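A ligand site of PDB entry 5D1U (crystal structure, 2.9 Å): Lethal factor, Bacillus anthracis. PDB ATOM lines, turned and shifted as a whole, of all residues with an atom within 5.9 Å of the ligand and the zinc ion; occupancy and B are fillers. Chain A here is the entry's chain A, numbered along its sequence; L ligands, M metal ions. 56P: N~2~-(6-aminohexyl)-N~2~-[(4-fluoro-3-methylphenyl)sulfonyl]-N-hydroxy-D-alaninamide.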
ATOM      1  N   ASP A  67      25.684  30.817   7.368  1.00  0.00           N
ATOM      2  CA  ASP A  67      25.446  29.798   8.390  1.00  0.00           C
ATOM      3  C   ASP A  67      26.719  29.013   8.718  1.00  0.00           C
ATOM      4  O   ASP A  67      27.112  28.934   9.875  1.00  0.00           O
ATOM      5  CB  ASP A  67      24.349  28.838   7.948  1.00  0.00           C
ATOM      6  N   PHE A  68      27.347  28.433   7.690  1.00  0.00           N
ATOM      7  CA  PHE A  68      28.476  27.524   7.891  1.00  0.00           C
ATOM      8  C   PHE A  68      29.855  28.169   7.727  1.00  0.00           C
ATOM      9  O   PHE A  68      30.879  27.552   8.017  1.00  0.00           O
ATOM     10  CB  PHE A  68      28.368  26.334   6.932  1.00  0.00           C
ATOM     11  N   VAL A 392      28.184  17.669   8.555  1.00  0.00           N
ATOM     12  CA  VAL A 392      28.063  18.898   9.296  1.00  0.00           C
ATOM     13  C   VAL A 392      28.848  18.882  10.597  1.00  0.00           C
ATOM     14  O   VAL A 392      28.880  17.848  11.261  1.00  0.00           O
ATOM     15  CB  VAL A 392      26.573  19.172   9.607  1.00  0.00           C
ATOM     16  CG1 VAL A 392      26.406  20.169  10.741  1.00  0.00           C
ATOM     17  CG2 VAL A 392      25.903  19.649   8.369  1.00  0.00           C
ATOM     18  N   HIS A 393      29.493  20.003  10.924  1.00  0.00           N
ATOM     19  CA  HIS A 393      30.040  20.255  12.268  1.00  0.00           C
ATOM     20  C   HIS A 393      29.328  21.454  12.928  1.00  0.00           C
ATOM     21  O   HIS A 393      29.033  22.427  12.234  1.00  0.00           O
ATOM     22  CB  HIS A 393      31.534  20.519  12.199  1.00  0.00           C
ATOM     23  CG  HIS A 393      32.138  20.931  13.507  1.00  0.00           C
ATOM     24  ND1 HIS A 393      31.907  20.252  14.678  1.00  0.00           N
ATOM     25  CD2 HIS A 393      32.956  21.966  13.824  1.00  0.00           C
ATOM     26  CE1 HIS A 393      32.560  20.837  15.669  1.00  0.00           C
ATOM     27  NE2 HIS A 393      33.197  21.881  15.181  1.00  0.00           N
ATOM     28  N   SER A 394      29.084  21.393  14.244  1.00  0.00           N
ATOM     29  CA  SER A 394      28.341  22.426  14.998  1.00  0.00           C
ATOM     30  C   SER A 394      28.148  22.005  16.465  1.00  0.00           C
ATOM     31  O   SER A 394      28.539  20.892  16.823  1.00  0.00           O
ATOM     32  CB  SER A 394      26.987  22.706  14.361  1.00  0.00           C
ATOM     33  OG  SER A 394      26.252  21.494  14.272  1.00  0.00           O
ATOM     34  N   LYS A 395      27.525  22.846  17.299  1.00  0.00           N
ATOM     35  CA  LYS A 395      27.418  22.594  18.748  1.00  0.00           C
ATOM     36  C   LYS A 395      26.714  21.279  19.063  1.00  0.00           C
ATOM     37  O   LYS A 395      27.045  20.593  20.032  1.00  0.00           O
ATOM     38  CB  LYS A 395      26.692  23.747  19.458  1.00  0.00           C
ATOM     39  N   GLY A 396      25.735  20.923  18.232  1.00  0.00           N
ATOM     40  CA  GLY A 396      25.005  19.694  18.445  1.00  0.00           C
ATOM     41  C   GLY A 396      24.273  19.216  17.207  1.00  0.00           C
ATOM     42  O   GLY A 396      24.167  19.943  16.224  1.00  0.00           O
ATOM     43  N   LEU A 397      23.764  17.986  17.245  1.00  0.00           N
ATOM     44  CA  LEU A 397      23.148  17.404  16.059  1.00  0.00           C
ATOM     45  C   LEU A 397      22.145  16.292  16.429  1.00  0.00           C
ATOM     46  O   LEU A 397      22.296  15.624  17.458  1.00  0.00           O
ATOM     47  CB  LEU A 397      24.241  16.841  15.126  1.00  0.00           C
ATOM     48  CG  LEU A 397      23.977  16.797  13.623  1.00  0.00           C
ATOM     49  CD1 LEU A 397      24.009  18.202  13.039  1.00  0.00           C
ATOM     50  CD2 LEU A 397      24.978  15.922  12.938  1.00  0.00           C
ATOM     51  N   TYR A 398      21.120  16.115  15.593  1.00  0.00           N
ATOM     52  CA  TYR A 398      20.356  14.877  15.667  1.00  0.00           C
ATOM     53  C   TYR A 398      20.444  14.130  14.345  1.00  0.00           C
ATOM     54  O   TYR A 398      20.195  14.677  13.267  1.00  0.00           O
ATOM     55  CB  TYR A 398      18.898  15.137  16.053  1.00  0.00           C
ATOM     56  CG  TYR A 398      18.083  13.847  16.129  1.00  0.00           C
ATOM     57  CD1 TYR A 398      18.279  12.937  17.159  1.00  0.00           C
ATOM     58  CD2 TYR A 398      17.166  13.519  15.139  1.00  0.00           C
ATOM     59  CE1 TYR A 398      17.587  11.770  17.222  1.00  0.00           C
ATOM     60  CE2 TYR A 398      16.460  12.348  15.193  1.00  0.00           C
ATOM     61  CZ  TYR A 398      16.666  11.474  16.236  1.00  0.00           C
ATOM     62  OH  TYR A 398      15.955  10.285  16.317  1.00  0.00           O
ATOM     63  N   LYS A 412      30.800  26.810  20.686  1.00  0.00           N
ATOM     64  CA  LYS A 412      29.627  27.541  21.131  1.00  0.00           C
ATOM     65  C   LYS A 412      28.667  27.774  19.972  1.00  0.00           C
ATOM     66  O   LYS A 412      29.024  28.369  18.947  1.00  0.00           O
ATOM     67  CB  LYS A 412      30.050  28.869  21.761  1.00  0.00           C
ATOM     68  CG  LYS A 412      28.886  29.699  22.322  1.00  0.00           C
ATOM     69  CD  LYS A 412      29.396  31.053  22.843  1.00  0.00           C
ATOM     70  CE  LYS A 412      28.262  31.973  23.311  1.00  0.00           C
ATOM     71  NZ  LYS A 412      28.681  33.418  23.349  1.00  0.00           N
ATOM     72  N   GLY A 413      27.439  27.300  20.125  1.00  0.00           N
ATOM     73  CA  GLY A 413      26.410  27.529  19.125  1.00  0.00           C
ATOM     74  C   GLY A 413      25.893  28.957  19.157  1.00  0.00           C
ATOM     75  O   GLY A 413      25.831  29.569  20.218  1.00  0.00           O
ATOM     76  N   VAL A 414      25.532  29.499  17.993  1.00  0.00           N
ATOM     77  CA  VAL A 414      25.039  30.866  17.961  1.00  0.00           C
ATOM     78  C   VAL A 414      23.670  30.926  18.609  1.00  0.00           C
ATOM     79  O   VAL A 414      22.773  30.175  18.228  1.00  0.00           O
ATOM     80  CB  VAL A 414      24.959  31.439  16.522  1.00  0.00           C
ATOM     81  CG1 VAL A 414      24.108  32.709  16.480  1.00  0.00           C
ATOM     82  CG2 VAL A 414      26.350  31.711  15.971  1.00  0.00           C
ATOM     83  N   GLU A 415      23.570  31.794  19.619  1.00  0.00           N
ATOM     84  CA  GLU A 415      22.351  32.116  20.338  1.00  0.00           C
ATOM     85  C   GLU A 415      22.072  31.055  21.420  1.00  0.00           C
ATOM     86  O   GLU A 415      20.916  30.866  21.828  1.00  0.00           O
ATOM     87  CB  GLU A 415      21.182  32.209  19.371  1.00  0.00           C
ATOM     88  CG  GLU A 415      21.050  33.496  18.590  1.00  0.00           C
ATOM     89  CD  GLU A 415      20.030  33.360  17.471  1.00  0.00           C
ATOM     90  OE1 GLU A 415      19.575  32.215  17.222  1.00  0.00           O
ATOM     91  OE2 GLU A 415      19.682  34.390  16.847  1.00  0.00           O
ATOM     92  N   LEU A 416      23.106  30.388  21.908  1.00  0.00           N
ATOM     93  CA  LEU A 416      22.894  29.456  23.004  1.00  0.00           C
ATOM     94  C   LEU A 416      23.596  29.956  24.237  1.00  0.00           C
ATOM     95  O   LEU A 416      24.775  30.267  24.150  1.00  0.00           O
ATOM     96  CB  LEU A 416      23.399  28.074  22.629  1.00  0.00           C
ATOM     97  CG  LEU A 416      22.468  27.292  21.701  1.00  0.00           C
ATOM     98  CD1 LEU A 416      23.058  25.959  21.304  1.00  0.00           C
ATOM     99  CD2 LEU A 416      21.133  27.110  22.386  1.00  0.00           C
ATOM    100  N   GLU A 421      21.441  24.028  26.971  1.00  0.00           N
ATOM    101  CA  GLU A 421      20.332  24.442  26.132  1.00  0.00           C
ATOM    102  C   GLU A 421      20.354  23.787  24.752  1.00  0.00           C
ATOM    103  O   GLU A 421      19.304  23.427  24.213  1.00  0.00           O
ATOM    104  CB  GLU A 421      20.301  25.970  26.000  1.00  0.00           C
ATOM    105  CG  GLU A 421      19.205  26.592  26.858  1.00  0.00           C
ATOM    106  CD  GLU A 421      19.370  28.075  27.082  1.00  0.00           C
ATOM    107  OE1 GLU A 421      20.118  28.720  26.305  1.00  0.00           O
ATOM    108  OE2 GLU A 421      18.742  28.592  28.040  1.00  0.00           O
ATOM    109  N   GLY A 422      21.550  23.589  24.199  1.00  0.00           N
ATOM    110  CA  GLY A 422      21.701  23.072  22.857  1.00  0.00           C
ATOM    111  C   GLY A 422      21.235  21.648  22.761  1.00  0.00           C
ATOM    112  O   GLY A 422      20.685  21.220  21.744  1.00  0.00           O
ATOM    113  N   PHE A 423      21.441  20.906  23.836  1.00  0.00           N
ATOM    114  CA  PHE A 423      20.959  19.539  23.934  1.00  0.00           C
ATOM    115  C   PHE A 423      19.442  19.490  23.776  1.00  0.00           C
ATOM    116  O   PHE A 423      18.918  18.737  22.951  1.00  0.00           O
ATOM    117  CB  PHE A 423      21.365  18.907  25.260  1.00  0.00           C
ATOM    118  CG  PHE A 423      21.175  17.428  25.298  1.00  0.00           C
ATOM    119  CD1 PHE A 423      22.153  16.583  24.798  1.00  0.00           C
ATOM    120  CD2 PHE A 423      20.011  16.867  25.810  1.00  0.00           C
ATOM    121  CE1 PHE A 423      21.984  15.203  24.816  1.00  0.00           C
ATOM    122  CE2 PHE A 423      19.832  15.489  25.831  1.00  0.00           C
ATOM    123  CZ  PHE A 423      20.820  14.655  25.322  1.00  0.00           C
ATOM    124  N   HIS A 425      17.489  21.523  22.450  1.00  0.00           N
ATOM    125  CA  HIS A 425      17.221  21.732  21.040  1.00  0.00           C
ATOM    126  C   HIS A 425      17.299  20.415  20.239  1.00  0.00           C
ATOM    127  O   HIS A 425      16.454  20.166  19.375  1.00  0.00           O
ATOM    128  CB  HIS A 425      18.169  22.767  20.430  1.00  0.00           C
ATOM    129  CG  HIS A 425      18.046  22.908  18.946  1.00  0.00           C
ATOM    130  ND1 HIS A 425      17.427  23.980  18.348  1.00  0.00           N
ATOM    131  CD2 HIS A 425      18.450  22.099  17.933  1.00  0.00           C
ATOM    132  CE1 HIS A 425      17.456  23.836  17.032  1.00  0.00           C
ATOM    133  NE2 HIS A 425      18.074  22.705  16.755  1.00  0.00           N
ATOM    134  N   GLU A 426      18.307  19.574  20.496  1.00  0.00           N
ATOM    135  CA  GLU A 426      18.450  18.312  19.737  1.00  0.00           C
ATOM    136  C   GLU A 426      17.397  17.279  20.106  1.00  0.00           C
ATOM    137  O   GLU A 426      16.826  16.628  19.246  1.00  0.00           O
ATOM    138  CB  GLU A 426      19.834  17.700  19.921  1.00  0.00           C
ATOM    139  CG  GLU A 426      21.010  18.628  19.633  1.00  0.00           C
ATOM    140  CD  GLU A 426      21.002  19.152  18.212  1.00  0.00           C
ATOM    141  OE1 GLU A 426      21.523  20.263  18.001  1.00  0.00           O
ATOM    142  OE2 GLU A 426      20.468  18.443  17.331  1.00  0.00           O
ATOM    143  N   HIS A 429      14.548  17.697  18.244  1.00  0.00           N
ATOM    144  CA  HIS A 429      14.558  16.979  16.963  1.00  0.00           C
ATOM    145  C   HIS A 429      14.111  15.503  17.097  1.00  0.00           C
ATOM    146  O   HIS A 429      13.460  14.965  16.191  1.00  0.00           O
ATOM    147  CB  HIS A 429      15.952  17.024  16.341  1.00  0.00           C
ATOM    148  CG  HIS A 429      16.307  18.333  15.719  1.00  0.00           C
ATOM    149  ND1 HIS A 429      15.569  18.920  14.718  1.00  0.00           N
ATOM    150  CD2 HIS A 429      17.372  19.154  15.923  1.00  0.00           C
ATOM    151  CE1 HIS A 429      16.150  20.049  14.345  1.00  0.00           C
ATOM    152  NE2 HIS A 429      17.242  20.217  15.061  1.00  0.00           N
ATOM    153  N   TYR A 467      17.273  32.088  14.011  1.00  0.00           N
ATOM    154  CA  TYR A 467      17.678  30.802  13.434  1.00  0.00           C
ATOM    155  C   TYR A 467      16.483  29.881  13.208  1.00  0.00           C
ATOM    156  O   TYR A 467      16.544  28.962  12.376  1.00  0.00           O
ATOM    157  CB  TYR A 467      18.724  30.116  14.320  1.00  0.00           C
ATOM    158  CG  TYR A 467      19.187  28.778  13.785  1.00  0.00           C
ATOM    159  CD1 TYR A 467      19.663  28.670  12.489  1.00  0.00           C
ATOM    160  CD2 TYR A 467      19.132  27.637  14.571  1.00  0.00           C
ATOM    161  CE1 TYR A 467      20.068  27.460  11.975  1.00  0.00           C
ATOM    162  CE2 TYR A 467      19.547  26.413  14.060  1.00  0.00           C
ATOM    163  CZ  TYR A 467      20.007  26.331  12.767  1.00  0.00           C
ATOM    164  OH  TYR A 467      20.427  25.125  12.229  1.00  0.00           O
ATOM    165  N   GLU A 474      13.786  22.901  12.168  1.00  0.00           N
ATOM    166  CA  GLU A 474      14.553  23.718  13.094  1.00  0.00           C
ATOM    167  C   GLU A 474      13.638  24.625  13.870  1.00  0.00           C
ATOM    168  O   GLU A 474      13.847  24.846  15.061  1.00  0.00           O
ATOM    169  CB  GLU A 474      15.610  24.547  12.363  1.00  0.00           C
ATOM    170  CG  GLU A 474      16.671  23.765  11.614  1.00  0.00           C
ATOM    171  CD  GLU A 474      17.597  23.002  12.531  1.00  0.00           C
ATOM    172  OE1 GLU A 474      18.253  23.639  13.366  1.00  0.00           O
ATOM    173  OE2 GLU A 474      17.700  21.768  12.390  1.00  0.00           O
ATOM    174  N   ALA A 477      12.320  22.713  16.554  1.00  0.00           N
ATOM    175  CA  ALA A 477      13.344  22.427  17.566  1.00  0.00           C
ATOM    176  C   ALA A 477      13.575  23.636  18.469  1.00  0.00           C
ATOM    177  O   ALA A 477      13.519  23.522  19.698  1.00  0.00           O
ATOM    178  CB  ALA A 477      14.645  22.013  16.921  1.00  0.00           C
ATOM    179  N   GLU A 478      13.823  24.783  17.862  1.00  0.00           N
ATOM    180  CA  GLU A 478      14.021  25.996  18.620  1.00  0.00           C
ATOM    181  C   GLU A 478      12.797  26.319  19.497  1.00  0.00           C
ATOM    182  O   GLU A 478      12.960  26.693  20.662  1.00  0.00           O
ATOM    183  CB  GLU A 478      14.364  27.163  17.689  1.00  0.00           C
ATOM    184  CG  GLU A 478      15.826  27.213  17.285  1.00  0.00           C
ATOM    185  CD  GLU A 478      16.739  27.701  18.417  1.00  0.00           C
ATOM    186  OE1 GLU A 478      17.421  28.742  18.250  1.00  0.00           O
ATOM    187  OE2 GLU A 478      16.795  27.035  19.481  1.00  0.00           O
ATOM    188  N   ARG A 481      12.895  24.156  22.306  1.00  0.00           N
ATOM    189  CA  ARG A 481      13.952  24.584  23.215  1.00  0.00           C
ATOM    190  C   ARG A 481      13.443  25.677  24.147  1.00  0.00           C
ATOM    191  O   ARG A 481      13.473  25.521  25.370  1.00  0.00           O
ATOM    192  CB  ARG A 481      15.161  25.083  22.434  1.00  0.00           C
ATOM    193  CG  ARG A 481      16.297  25.546  23.305  1.00  0.00           C
ATOM    194  CD  ARG A 481      17.496  25.957  22.502  1.00  0.00           C
ATOM    195  NE  ARG A 481      17.278  27.194  21.744  1.00  0.00           N
ATOM    196  CZ  ARG A 481      17.354  28.413  22.268  1.00  0.00           C
ATOM    197  NH1 ARG A 481      17.619  28.593  23.562  1.00  0.00           N
ATOM    198  NH2 ARG A 481      17.150  29.472  21.477  1.00  0.00           N
HETATM  199  C1  56P L   1      23.139  22.640  14.275  1.00  0.00           C
HETATM  200  C2  56P L   1      21.697  22.198  14.470  1.00  0.00           C
HETATM  201  C20 56P L   1      23.935  26.343  11.617  1.00  0.00           C
HETATM  202  O5  56P L   1      20.216  20.474  15.024  1.00  0.00           O
HETATM  203  N6  56P L   1      23.508  24.035  14.625  1.00  0.00           N
HETATM  204  C10 56P L   1      22.899  24.666  17.041  1.00  0.00           C
HETATM  205  C11 56P L   1      22.259  25.902  17.156  1.00  0.00           C
HETATM  206  C12 56P L   1      21.211  26.054  18.042  1.00  0.00           C
HETATM  207  C13 56P L   1      20.783  24.987  18.814  1.00  0.00           C
HETATM  208  C14 56P L   1      21.418  23.758  18.714  1.00  0.00           C
HETATM  209  C15 56P L   1      22.464  23.596  17.824  1.00  0.00           C
HETATM  210  C19 56P L   1      24.384  25.566  12.852  1.00  0.00           C
HETATM  211  C18 56P L   1      23.169  24.960  13.535  1.00  0.00           C
HETATM  212  C28 56P L   1      23.444  22.319  12.810  1.00  0.00           C
HETATM  213  N4  56P L   1      21.518  20.973  14.963  1.00  0.00           N
HETATM  214  O3  56P L   1      20.734  22.879  14.136  1.00  0.00           O
HETATM  215  S7  56P L   1      24.116  24.452  16.011  1.00  0.00           S
HETATM  216  O8  56P L   1      24.923  25.659  15.992  1.00  0.00           O
HETATM  217  O9  56P L   1      24.932  23.402  16.549  1.00  0.00           O
HETATM  218  F16 56P L   1      19.759  25.155  19.668  1.00  0.00           F
HETATM  219  C17 56P L   1      20.516  27.389  18.167  1.00  0.00           C
HETATM  220 ZN    ZN M   1      18.684  21.697  14.926  1.00  0.00          ZN
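An oxygen (O3) of the ligand lies close to the side-chain hydroxyl of Tyr 467 (3.0 Å).
O9 of the ligand is in hydrogen-bond range of N of Gly 396 (3.1 Å).
OE1 of Glu 426 lies within hydrogen-bond range of N4 of the ligand (3.1 Å).
OG of Ser 394 lies close to O9 of the ligand (3.3 Å).
O9 of the ligand sits at hydrogen-bond distance from N of Lys 395, 2.8 Å away.
O of Gly 396 sits at hydrogen-bond distance from N4 of the ligand (3.1 Å).
The side-chain carboxylate (OE1) of Glu 421 is in salt-bridge range of the guanidinium group (NH1) of Arg 481 (3.7 Å).
The side-chain carboxylate (OE2) of Glu 426 is in hydrogen-bond range of the backbone NH (N) of Tyr 398.
OG of Ser 394 is in hydrogen-bond range of O of Gly 396, 3.3 Å away.
OE1 of Glu 426 lies close to N of Leu 397 (3.3 Å).
The side-chain carboxylate of Glu 474 sits close to the side-chain hydroxyl of Tyr 467 (2.9 Å).
A ring nitrogen (ND1) of His 425 is in hydrogen-bond range of the side-chain carboxylate (OE2) of Glu 478, 3.3 Å away.
The side-chain carboxylate (OE2) of Glu 478 lies within salt-bridge range of the guanidinium group (NH2) of Arg 481 (3.2 Å).
Gly 413 touches the ligand (CA to O8, 3.9 Å).
Val 414 touches the ligand.
Leu 416 touches the ligand.
OE1 of Glu 478 touches C17 of the ligand (3.4 Å).
Arg 481 touches the ligand.
Hydrophobic or aromatic side chains that line the ligand: Leu 416, His 425, His 429 and Tyr 467.
Along chain A the residues within 4 Å of the ligand span positions 394 to 481.
The nearest printed residue that does not touch the ligand is Gly 422 (4.02 Å).
Three residues have an atom within 4 Å of the zinc ion: His 425, His 429 and Glu 474.
The zinc ion is bound by an oxygen (O5) of the ligand (2.0 Å).
NE2 of His 429 is bound to the zinc ion.
The zinc ion is bound by a ring nitrogen (NE2) of His 425 (2.2 Å).
The zinc ion is bound by an oxygen (O3) of the ligand (2.5 Å).
OE1 of Glu 474 binds the zinc ion (2.5 Å).
The zinc ion has five donor atoms within binding distance.
Slightly farther from the zinc ion lies the side-chain carboxylate (OE2) of Glu 474 (2.7 Å).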
